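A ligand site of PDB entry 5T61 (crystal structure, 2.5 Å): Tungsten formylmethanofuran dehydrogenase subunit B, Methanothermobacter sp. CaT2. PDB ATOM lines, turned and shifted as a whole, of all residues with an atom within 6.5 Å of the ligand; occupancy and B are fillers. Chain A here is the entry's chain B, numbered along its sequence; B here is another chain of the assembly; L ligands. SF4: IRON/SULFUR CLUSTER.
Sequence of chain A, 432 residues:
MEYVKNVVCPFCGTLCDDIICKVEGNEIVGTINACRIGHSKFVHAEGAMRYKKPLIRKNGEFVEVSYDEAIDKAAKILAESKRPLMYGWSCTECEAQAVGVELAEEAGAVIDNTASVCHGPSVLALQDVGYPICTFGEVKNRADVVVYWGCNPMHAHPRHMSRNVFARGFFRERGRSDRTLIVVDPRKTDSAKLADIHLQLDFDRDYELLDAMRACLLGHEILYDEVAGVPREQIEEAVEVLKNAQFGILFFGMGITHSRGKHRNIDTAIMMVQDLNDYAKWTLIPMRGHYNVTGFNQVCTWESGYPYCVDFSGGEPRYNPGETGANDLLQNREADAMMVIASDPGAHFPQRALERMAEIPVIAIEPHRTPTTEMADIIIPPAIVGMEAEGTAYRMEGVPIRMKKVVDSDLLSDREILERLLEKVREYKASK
FE2 of the ligand is bound by SG of Cys 12, at 2.1 Å. The side-chain sulfur of Cys 9 binds an iron atom (FE4) of the ligand (2.6 Å). The backbone NH (N) of Cys 16 lies close to a sulfur (S3) of the ligand (3.8 Å). An iron atom (FE1) of the ligand is bound by the side-chain sulfur (SG) of Cys 16, at 2.7 Å. SG of Cys 35 binds FE3 of the ligand, at 2.7 Å.
Thr 14 of chain A touches the ligand. Leu 15 touches the ligand (N to S3, 3.9 Å). Gly 38 touches the ligand (CA to FE4, 3.97 Å). Arg 159 touches the ligand.
SG of Cys 12 sits close to OG1 of Thr 14 of chain A. The backbone carbonyl oxygen (O) of Cys 16 sits at hydrogen-bond distance from the backbone NH (N) of Cys 9. The guanidinium group of Arg 159 lies close to the side-chain sulfur of Cys 16 (3.2 Å). The guanidinium group (NE) of Arg 163 sits close to the side-chain sulfur (SG) of Cys 16, 3.1 Å away. The side-chain hydroxyl (OG1) of Thr 14 of chain A is in hydrogen-bond range of a ring nitrogen (ND1) of His 157 (3.2 Å). The guanidinium group of Arg 163 sits at hydrogen-bond distance from the backbone carbonyl oxygen of Thr 14 of chain A (3.4 Å). NE of Arg 159 sits at hydrogen-bond distance from O of Asn 33 (3.0 Å). NH1 of Arg 159 lies within salt-bridge range of OD1 of Asp 18.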
ATOM      1  N   CYS A   9     -31.922  -0.442   7.352  1.00  0.00           N
ATOM      2  CA  CYS A   9     -31.956  -0.428   5.881  1.00  0.00           C
ATOM      3  C   CYS A   9     -33.192  -1.150   5.355  1.00  0.00           C
ATOM      4  O   CYS A   9     -33.495  -2.262   5.797  1.00  0.00           O
ATOM      5  CB  CYS A   9     -30.720  -1.056   5.275  1.00  0.00           C
ATOM      6  SG  CYS A   9     -30.789  -0.966   3.464  1.00  0.00           S
ATOM      7  N   PRO A  10     -33.937  -0.533   4.414  1.00  0.00           N
ATOM      8  CA  PRO A  10     -35.171  -1.125   3.882  1.00  0.00           C
ATOM      9  C   PRO A  10     -34.998  -1.929   2.594  1.00  0.00           C
ATOM     10  O   PRO A  10     -35.666  -1.683   1.585  1.00  0.00           O
ATOM     11  CB  PRO A  10     -36.051   0.109   3.649  1.00  0.00           C
ATOM     12  CG  PRO A  10     -35.068   1.251   3.394  1.00  0.00           C
ATOM     13  CD  PRO A  10     -33.717   0.835   3.911  1.00  0.00           C
ATOM     14  N   PHE A  11     -34.092  -2.904   2.609  1.00  0.00           N
ATOM     15  CA  PHE A  11     -34.074  -3.800   1.446  1.00  0.00           C
ATOM     16  C   PHE A  11     -34.333  -5.252   1.824  1.00  0.00           C
ATOM     17  O   PHE A  11     -35.459  -5.743   1.657  1.00  0.00           O
ATOM     18  CB  PHE A  11     -32.780  -3.709   0.655  1.00  0.00           C
ATOM     19  CG  PHE A  11     -32.803  -4.531  -0.606  1.00  0.00           C
ATOM     20  CD1 PHE A  11     -33.550  -4.123  -1.705  1.00  0.00           C
ATOM     21  CD2 PHE A  11     -32.102  -5.724  -0.682  1.00  0.00           C
ATOM     22  CE1 PHE A  11     -33.590  -4.891  -2.859  1.00  0.00           C
ATOM     23  CE2 PHE A  11     -32.143  -6.492  -1.835  1.00  0.00           C
ATOM     24  CZ  PHE A  11     -32.884  -6.069  -2.930  1.00  0.00           C
ATOM     25  N   CYS A  12     -33.326  -5.963   2.317  1.00  0.00           N
ATOM     26  CA  CYS A  12     -33.499  -7.398   2.478  1.00  0.00           C
ATOM     27  C   CYS A  12     -33.708  -7.761   3.943  1.00  0.00           C
ATOM     28  O   CYS A  12     -33.592  -6.928   4.848  1.00  0.00           O
ATOM     29  CB  CYS A  12     -32.304  -8.189   1.918  1.00  0.00           C
ATOM     30  SG  CYS A  12     -30.840  -8.200   2.959  1.00  0.00           S
ATOM     31  N   GLY A  13     -34.022  -9.036   4.177  1.00  0.00           N
ATOM     32  CA  GLY A  13     -34.373  -9.538   5.499  1.00  0.00           C
ATOM     33  C   GLY A  13     -33.244  -9.521   6.502  1.00  0.00           C
ATOM     34  O   GLY A  13     -33.475  -9.845   7.670  1.00  0.00           O
ATOM     35  N   THR A  14     -32.018  -9.172   6.078  1.00  0.00           N
ATOM     36  CA  THR A  14     -30.944  -8.943   7.048  1.00  0.00           C
ATOM     37  C   THR A  14     -31.278  -7.776   7.966  1.00  0.00           C
ATOM     38  O   THR A  14     -30.912  -7.790   9.155  1.00  0.00           O
ATOM     39  CB  THR A  14     -29.622  -8.687   6.325  1.00  0.00           C
ATOM     40  OG1 THR A  14     -29.399  -9.697   5.343  1.00  0.00           O
ATOM     41  CG2 THR A  14     -28.466  -8.680   7.313  1.00  0.00           C
ATOM     42  N   LEU A  15     -31.990  -6.779   7.461  1.00  0.00           N
ATOM     43  CA  LEU A  15     -32.489  -5.632   8.217  1.00  0.00           C
ATOM     44  C   LEU A  15     -31.398  -5.025   9.095  1.00  0.00           C
ATOM     45  O   LEU A  15     -31.588  -4.788  10.292  1.00  0.00           O
ATOM     46  CB  LEU A  15     -33.702  -6.044   9.055  1.00  0.00           C
ATOM     47  CG  LEU A  15     -34.602  -4.900   9.536  1.00  0.00           C
ATOM     48  CD1 LEU A  15     -35.264  -4.238   8.342  1.00  0.00           C
ATOM     49  CD2 LEU A  15     -35.625  -5.386  10.547  1.00  0.00           C
ATOM     50  N   CYS A  16     -30.254  -4.743   8.480  1.00  0.00           N
ATOM     51  CA  CYS A  16     -29.189  -4.047   9.203  1.00  0.00           C
ATOM     52  C   CYS A  16     -29.689  -2.711   9.743  1.00  0.00           C
ATOM     53  O   CYS A  16     -30.382  -1.957   9.047  1.00  0.00           O
ATOM     54  CB  CYS A  16     -27.971  -3.831   8.310  1.00  0.00           C
ATOM     55  SG  CYS A  16     -26.950  -5.300   8.109  1.00  0.00           S
ATOM     56  N   ASP A  17     -29.326  -2.422  10.988  1.00  0.00           N
ATOM     57  CA  ASP A  17     -29.764  -1.205  11.664  1.00  0.00           C
ATOM     58  C   ASP A  17     -28.593  -0.326  12.099  1.00  0.00           C
ATOM     59  O   ASP A  17     -28.722   0.460  13.037  1.00  0.00           O
ATOM     60  CB  ASP A  17     -30.650  -1.536  12.869  1.00  0.00           C
ATOM     61  CG  ASP A  17     -29.881  -2.205  13.993  1.00  0.00           C
ATOM     62  OD1 ASP A  17     -29.159  -3.189  13.718  1.00  0.00           O
ATOM     63  OD2 ASP A  17     -30.006  -1.758  15.149  1.00  0.00           O
ATOM     64  N   ASP A  18     -27.432  -0.453  11.439  1.00  0.00           N
ATOM     65  CA  ASP A  18     -26.270   0.361  11.756  1.00  0.00           C
ATOM     66  C   ASP A  18     -25.887   1.256  10.586  1.00  0.00           C
ATOM     67  O   ASP A  18     -24.736   1.717  10.513  1.00  0.00           O
ATOM     68  CB  ASP A  18     -25.078  -0.518  12.154  1.00  0.00           C
ATOM     69  CG  ASP A  18     -24.574  -1.403  11.021  1.00  0.00           C
ATOM     70  OD1 ASP A  18     -25.280  -1.565  10.005  1.00  0.00           O
ATOM     71  OD2 ASP A  18     -23.451  -1.941  11.152  1.00  0.00           O
ATOM     72  N   ILE A  19     -26.826   1.519   9.676  1.00  0.00           N
ATOM     73  CA  ILE A  19     -26.535   2.326   8.501  1.00  0.00           C
ATOM     74  C   ILE A  19     -26.363   3.782   8.900  1.00  0.00           C
ATOM     75  O   ILE A  19     -27.123   4.322   9.726  1.00  0.00           O
ATOM     76  CB  ILE A  19     -27.658   2.179   7.457  1.00  0.00           C
ATOM     77  CG1 ILE A  19     -27.900   0.707   7.119  1.00  0.00           C
ATOM     78  CG2 ILE A  19     -27.343   3.002   6.213  1.00  0.00           C
ATOM     79  CD1 ILE A  19     -26.641  -0.060   6.803  1.00  0.00           C
ATOM     80  N   ASN A  33     -21.523   1.863   5.619  1.00  0.00           N
ATOM     81  CA  ASN A  33     -21.770   0.528   6.148  1.00  0.00           C
ATOM     82  C   ASN A  33     -22.785  -0.271   5.339  1.00  0.00           C
ATOM     83  O   ASN A  33     -22.722  -1.503   5.321  1.00  0.00           O
ATOM     84  CB  ASN A  33     -22.234   0.596   7.613  1.00  0.00           C
ATOM     85  CG  ASN A  33     -21.187   1.191   8.519  1.00  0.00           C
ATOM     86  OD1 ASN A  33     -19.988   1.050   8.294  1.00  0.00           O
ATOM     87  ND2 ASN A  33     -21.641   1.892   9.551  1.00  0.00           N
ATOM     88  N   ALA A  34     -23.720   0.407   4.677  1.00  0.00           N
ATOM     89  CA  ALA A  34     -24.666  -0.276   3.813  1.00  0.00           C
ATOM     90  C   ALA A  34     -23.949  -0.940   2.645  1.00  0.00           C
ATOM     91  O   ALA A  34     -22.956  -0.419   2.129  1.00  0.00           O
ATOM     92  CB  ALA A  34     -25.723   0.706   3.295  1.00  0.00           C
ATOM     93  N   CYS A  35     -24.461  -2.095   2.224  1.00  0.00           N
ATOM     94  CA  CYS A  35     -23.828  -2.791   1.123  1.00  0.00           C
ATOM     95  C   CYS A  35     -24.225  -2.128  -0.200  1.00  0.00           C
ATOM     96  O   CYS A  35     -24.948  -1.130  -0.226  1.00  0.00           O
ATOM     97  CB  CYS A  35     -24.224  -4.266   1.086  1.00  0.00           C
ATOM     98  SG  CYS A  35     -25.705  -4.535   0.108  1.00  0.00           S
ATOM     99  N   ARG A  36     -23.782  -2.727  -1.313  1.00  0.00           N
ATOM    100  CA  ARG A  36     -24.028  -2.124  -2.616  1.00  0.00           C
ATOM    101  C   ARG A  36     -25.525  -1.987  -2.900  1.00  0.00           C
ATOM    102  O   ARG A  36     -25.955  -0.997  -3.487  1.00  0.00           O
ATOM    103  CB  ARG A  36     -23.358  -2.943  -3.716  1.00  0.00           C
ATOM    104  CG  ARG A  36     -23.656  -2.410  -5.116  1.00  0.00           C
ATOM    105  CD  ARG A  36     -22.956  -3.176  -6.234  1.00  0.00           C
ATOM    106  NE  ARG A  36     -21.496  -3.045  -6.206  1.00  0.00           N
ATOM    107  CZ  ARG A  36     -20.830  -2.073  -6.801  1.00  0.00           C
ATOM    108  NH1 ARG A  36     -21.490  -1.126  -7.458  1.00  0.00           N
ATOM    109  NH2 ARG A  36     -19.512  -2.037  -6.744  1.00  0.00           N
ATOM    110  N   ILE A  37     -26.317  -2.973  -2.472  1.00  0.00           N
ATOM    111  CA  ILE A  37     -27.752  -2.911  -2.751  1.00  0.00           C
ATOM    112  C   ILE A  37     -28.413  -1.858  -1.875  1.00  0.00           C
ATOM    113  O   ILE A  37     -29.079  -0.939  -2.369  1.00  0.00           O
ATOM    114  CB  ILE A  37     -28.404  -4.288  -2.548  1.00  0.00           C
ATOM    115  CG1 ILE A  37     -27.644  -5.383  -3.291  1.00  0.00           C
ATOM    116  CG2 ILE A  37     -29.836  -4.251  -3.040  1.00  0.00           C
ATOM    117  CD1 ILE A  37     -28.085  -6.772  -2.895  1.00  0.00           C
ATOM    118  N   GLY A  38     -28.239  -1.985  -0.555  1.00  0.00           N
ATOM    119  CA  GLY A  38     -28.838  -1.019   0.362  1.00  0.00           C
ATOM    120  C   GLY A  38     -28.504   0.411  -0.006  1.00  0.00           C
ATOM    121  O   GLY A  38     -29.360   1.291   0.072  1.00  0.00           O
ATOM    122  N   HIS A  39     -27.255   0.665  -0.384  1.00  0.00           N
ATOM    123  CA  HIS A  39     -26.869   1.999  -0.844  1.00  0.00           C
ATOM    124  C   HIS A  39     -27.701   2.445  -2.042  1.00  0.00           C
ATOM    125  O   HIS A  39     -28.119   3.606  -2.109  1.00  0.00           O
ATOM    126  CB  HIS A  39     -25.378   2.015  -1.191  1.00  0.00           C
ATOM    127  CG  HIS A  39     -24.943   3.258  -1.905  1.00  0.00           C
ATOM    128  ND1 HIS A  39     -24.689   4.446  -1.242  1.00  0.00           N
ATOM    129  CD2 HIS A  39     -24.714   3.495  -3.214  1.00  0.00           C
ATOM    130  CE1 HIS A  39     -24.331   5.359  -2.118  1.00  0.00           C
ATOM    131  NE2 HIS A  39     -24.337   4.816  -3.327  1.00  0.00           N
ATOM    132  N   PHE A  42     -31.076   3.818  -0.917  1.00  0.00           N
ATOM    133  CA  PHE A  42     -31.032   5.095  -0.219  1.00  0.00           C
ATOM    134  C   PHE A  42     -30.772   6.261  -1.168  1.00  0.00           C
ATOM    135  O   PHE A  42     -31.273   7.366  -0.930  1.00  0.00           O
ATOM    136  CB  PHE A  42     -29.964   5.064   0.877  1.00  0.00           C
ATOM    137  CG  PHE A  42     -30.408   4.408   2.143  1.00  0.00           C
ATOM    138  CD1 PHE A  42     -31.298   5.027   3.001  1.00  0.00           C
ATOM    139  CD2 PHE A  42     -29.902   3.161   2.502  1.00  0.00           C
ATOM    140  CE1 PHE A  42     -31.693   4.425   4.174  1.00  0.00           C
ATOM    141  CE2 PHE A  42     -30.309   2.549   3.675  1.00  0.00           C
ATOM    142  CZ  PHE A  42     -31.200   3.182   4.514  1.00  0.00           C
ATOM    143  N   ALA A 156     -27.368 -11.896  -2.271  1.00  0.00           N
ATOM    144  CA  ALA A 156     -28.741 -11.667  -1.861  1.00  0.00           C
ATOM    145  C   ALA A 156     -28.917 -11.137  -0.445  1.00  0.00           C
ATOM    146  O   ALA A 156     -29.971 -10.573  -0.141  1.00  0.00           O
ATOM    147  CB  ALA A 156     -29.557 -12.966  -1.998  1.00  0.00           C
ATOM    148  N   HIS A 157     -27.919 -11.327   0.436  1.00  0.00           N
ATOM    149  CA  HIS A 157     -27.905 -10.705   1.762  1.00  0.00           C
ATOM    150  C   HIS A 157     -26.469 -10.313   2.067  1.00  0.00           C
ATOM    151  O   HIS A 157     -25.833 -10.887   2.956  1.00  0.00           O
ATOM    152  CB  HIS A 157     -28.462 -11.656   2.823  1.00  0.00           C
ATOM    153  CG  HIS A 157     -29.874 -12.077   2.578  1.00  0.00           C
ATOM    154  ND1 HIS A 157     -30.947 -11.491   3.233  1.00  0.00           N
ATOM    155  CD2 HIS A 157     -30.406 -13.019   1.760  1.00  0.00           C
ATOM    156  CE1 HIS A 157     -32.069 -12.052   2.814  1.00  0.00           C
ATOM    157  NE2 HIS A 157     -31.768 -12.980   1.924  1.00  0.00           N
ATOM    158  N   PRO A 158     -25.939  -9.343   1.334  1.00  0.00           N
ATOM    159  CA  PRO A 158     -24.471  -9.188   1.246  1.00  0.00           C
ATOM    160  C   PRO A 158     -23.757  -9.080   2.583  1.00  0.00           C
ATOM    161  O   PRO A 158     -22.643  -9.597   2.719  1.00  0.00           O
ATOM    162  CB  PRO A 158     -24.317  -7.905   0.421  1.00  0.00           C
ATOM    163  CG  PRO A 158     -25.537  -7.901  -0.437  1.00  0.00           C
ATOM    164  CD  PRO A 158     -26.636  -8.406   0.444  1.00  0.00           C
ATOM    165  N   ARG A 159     -24.368  -8.477   3.596  1.00  0.00           N
ATOM    166  CA  ARG A 159     -23.716  -8.339   4.888  1.00  0.00           C
ATOM    167  C   ARG A 159     -24.050  -9.480   5.845  1.00  0.00           C
ATOM    168  O   ARG A 159     -23.625  -9.444   6.994  1.00  0.00           O
ATOM    169  CB  ARG A 159     -24.075  -6.995   5.526  1.00  0.00           C
ATOM    170  CG  ARG A 159     -23.750  -5.786   4.665  1.00  0.00           C
ATOM    171  CD  ARG A 159     -24.103  -4.495   5.392  1.00  0.00           C
ATOM    172  NE  ARG A 159     -23.220  -4.247   6.520  1.00  0.00           N
ATOM    173  CZ  ARG A 159     -23.553  -3.537   7.592  1.00  0.00           C
ATOM    174  NH1 ARG A 159     -24.759  -3.009   7.689  1.00  0.00           N
ATOM    175  NH2 ARG A 159     -22.676  -3.348   8.579  1.00  0.00           N
ATOM    176  N   HIS A 160     -24.793 -10.489   5.386  1.00  0.00           N
ATOM    177  CA  HIS A 160     -25.228 -11.565   6.272  1.00  0.00           C
ATOM    178  C   HIS A 160     -24.038 -12.342   6.845  1.00  0.00           C
ATOM    179  O   HIS A 160     -24.008 -12.650   8.033  1.00  0.00           O
ATOM    180  CB  HIS A 160     -26.172 -12.507   5.524  1.00  0.00           C
ATOM    181  CG  HIS A 160     -27.038 -13.339   6.423  1.00  0.00           C
ATOM    182  ND1 HIS A 160     -26.632 -14.543   6.967  1.00  0.00           N
ATOM    183  CD2 HIS A 160     -28.313 -13.150   6.851  1.00  0.00           C
ATOM    184  CE1 HIS A 160     -27.609 -15.050   7.691  1.00  0.00           C
ATOM    185  NE2 HIS A 160     -28.637 -14.227   7.643  1.00  0.00           N
ATOM    186  N   ARG A 163     -21.812 -10.284   9.381  1.00  0.00           N
ATOM    187  CA  ARG A 163     -22.416 -10.067  10.689  1.00  0.00           C
ATOM    188  C   ARG A 163     -22.588 -11.362  11.491  1.00  0.00           C
ATOM    189  O   ARG A 163     -22.559 -11.323  12.723  1.00  0.00           O
ATOM    190  CB  ARG A 163     -23.750  -9.329  10.546  1.00  0.00           C
ATOM    191  CG  ARG A 163     -23.641  -8.091   9.675  1.00  0.00           C
ATOM    192  CD  ARG A 163     -24.612  -7.006  10.080  1.00  0.00           C
ATOM    193  NE  ARG A 163     -25.997  -7.461  10.190  1.00  0.00           N
ATOM    194  CZ  ARG A 163     -26.864  -6.925  11.041  1.00  0.00           C
ATOM    195  NH1 ARG A 163     -26.425  -6.072  11.969  1.00  0.00           N
ATOM    196  NH2 ARG A 163     -28.120  -7.347  11.091  1.00  0.00           N
ATOM    197  N   GLY B  14     -19.788  -4.488  -1.228  1.00  0.00           N
ATOM    198  CA  GLY B  14     -20.121  -3.856   0.032  1.00  0.00           C
ATOM    199  C   GLY B  14     -20.437  -4.821   1.149  1.00  0.00           C
ATOM    200  O   GLY B  14     -21.065  -4.431   2.143  1.00  0.00           O
HETATM  201 FE1  SF4 L   1     -27.879  -5.088   5.587  1.00  0.00          FE
HETATM  202 FE2  SF4 L   1     -29.695  -6.478   3.269  1.00  0.00          FE
HETATM  203 FE3  SF4 L   1     -26.996  -4.824   2.493  1.00  0.00          FE
HETATM  204 FE4  SF4 L   1     -29.582  -3.272   3.543  1.00  0.00          FE
HETATM  205  S1  SF4 L   1     -29.073  -4.784   2.207  1.00  0.00           S
HETATM  206  S2  SF4 L   1     -27.609  -3.632   4.100  1.00  0.00           S
HETATM  207  S3  SF4 L   1     -29.789  -4.992   4.721  1.00  0.00           S
HETATM  208  S4  SF4 L   1     -27.690  -6.242   3.859  1.00  0.00           S
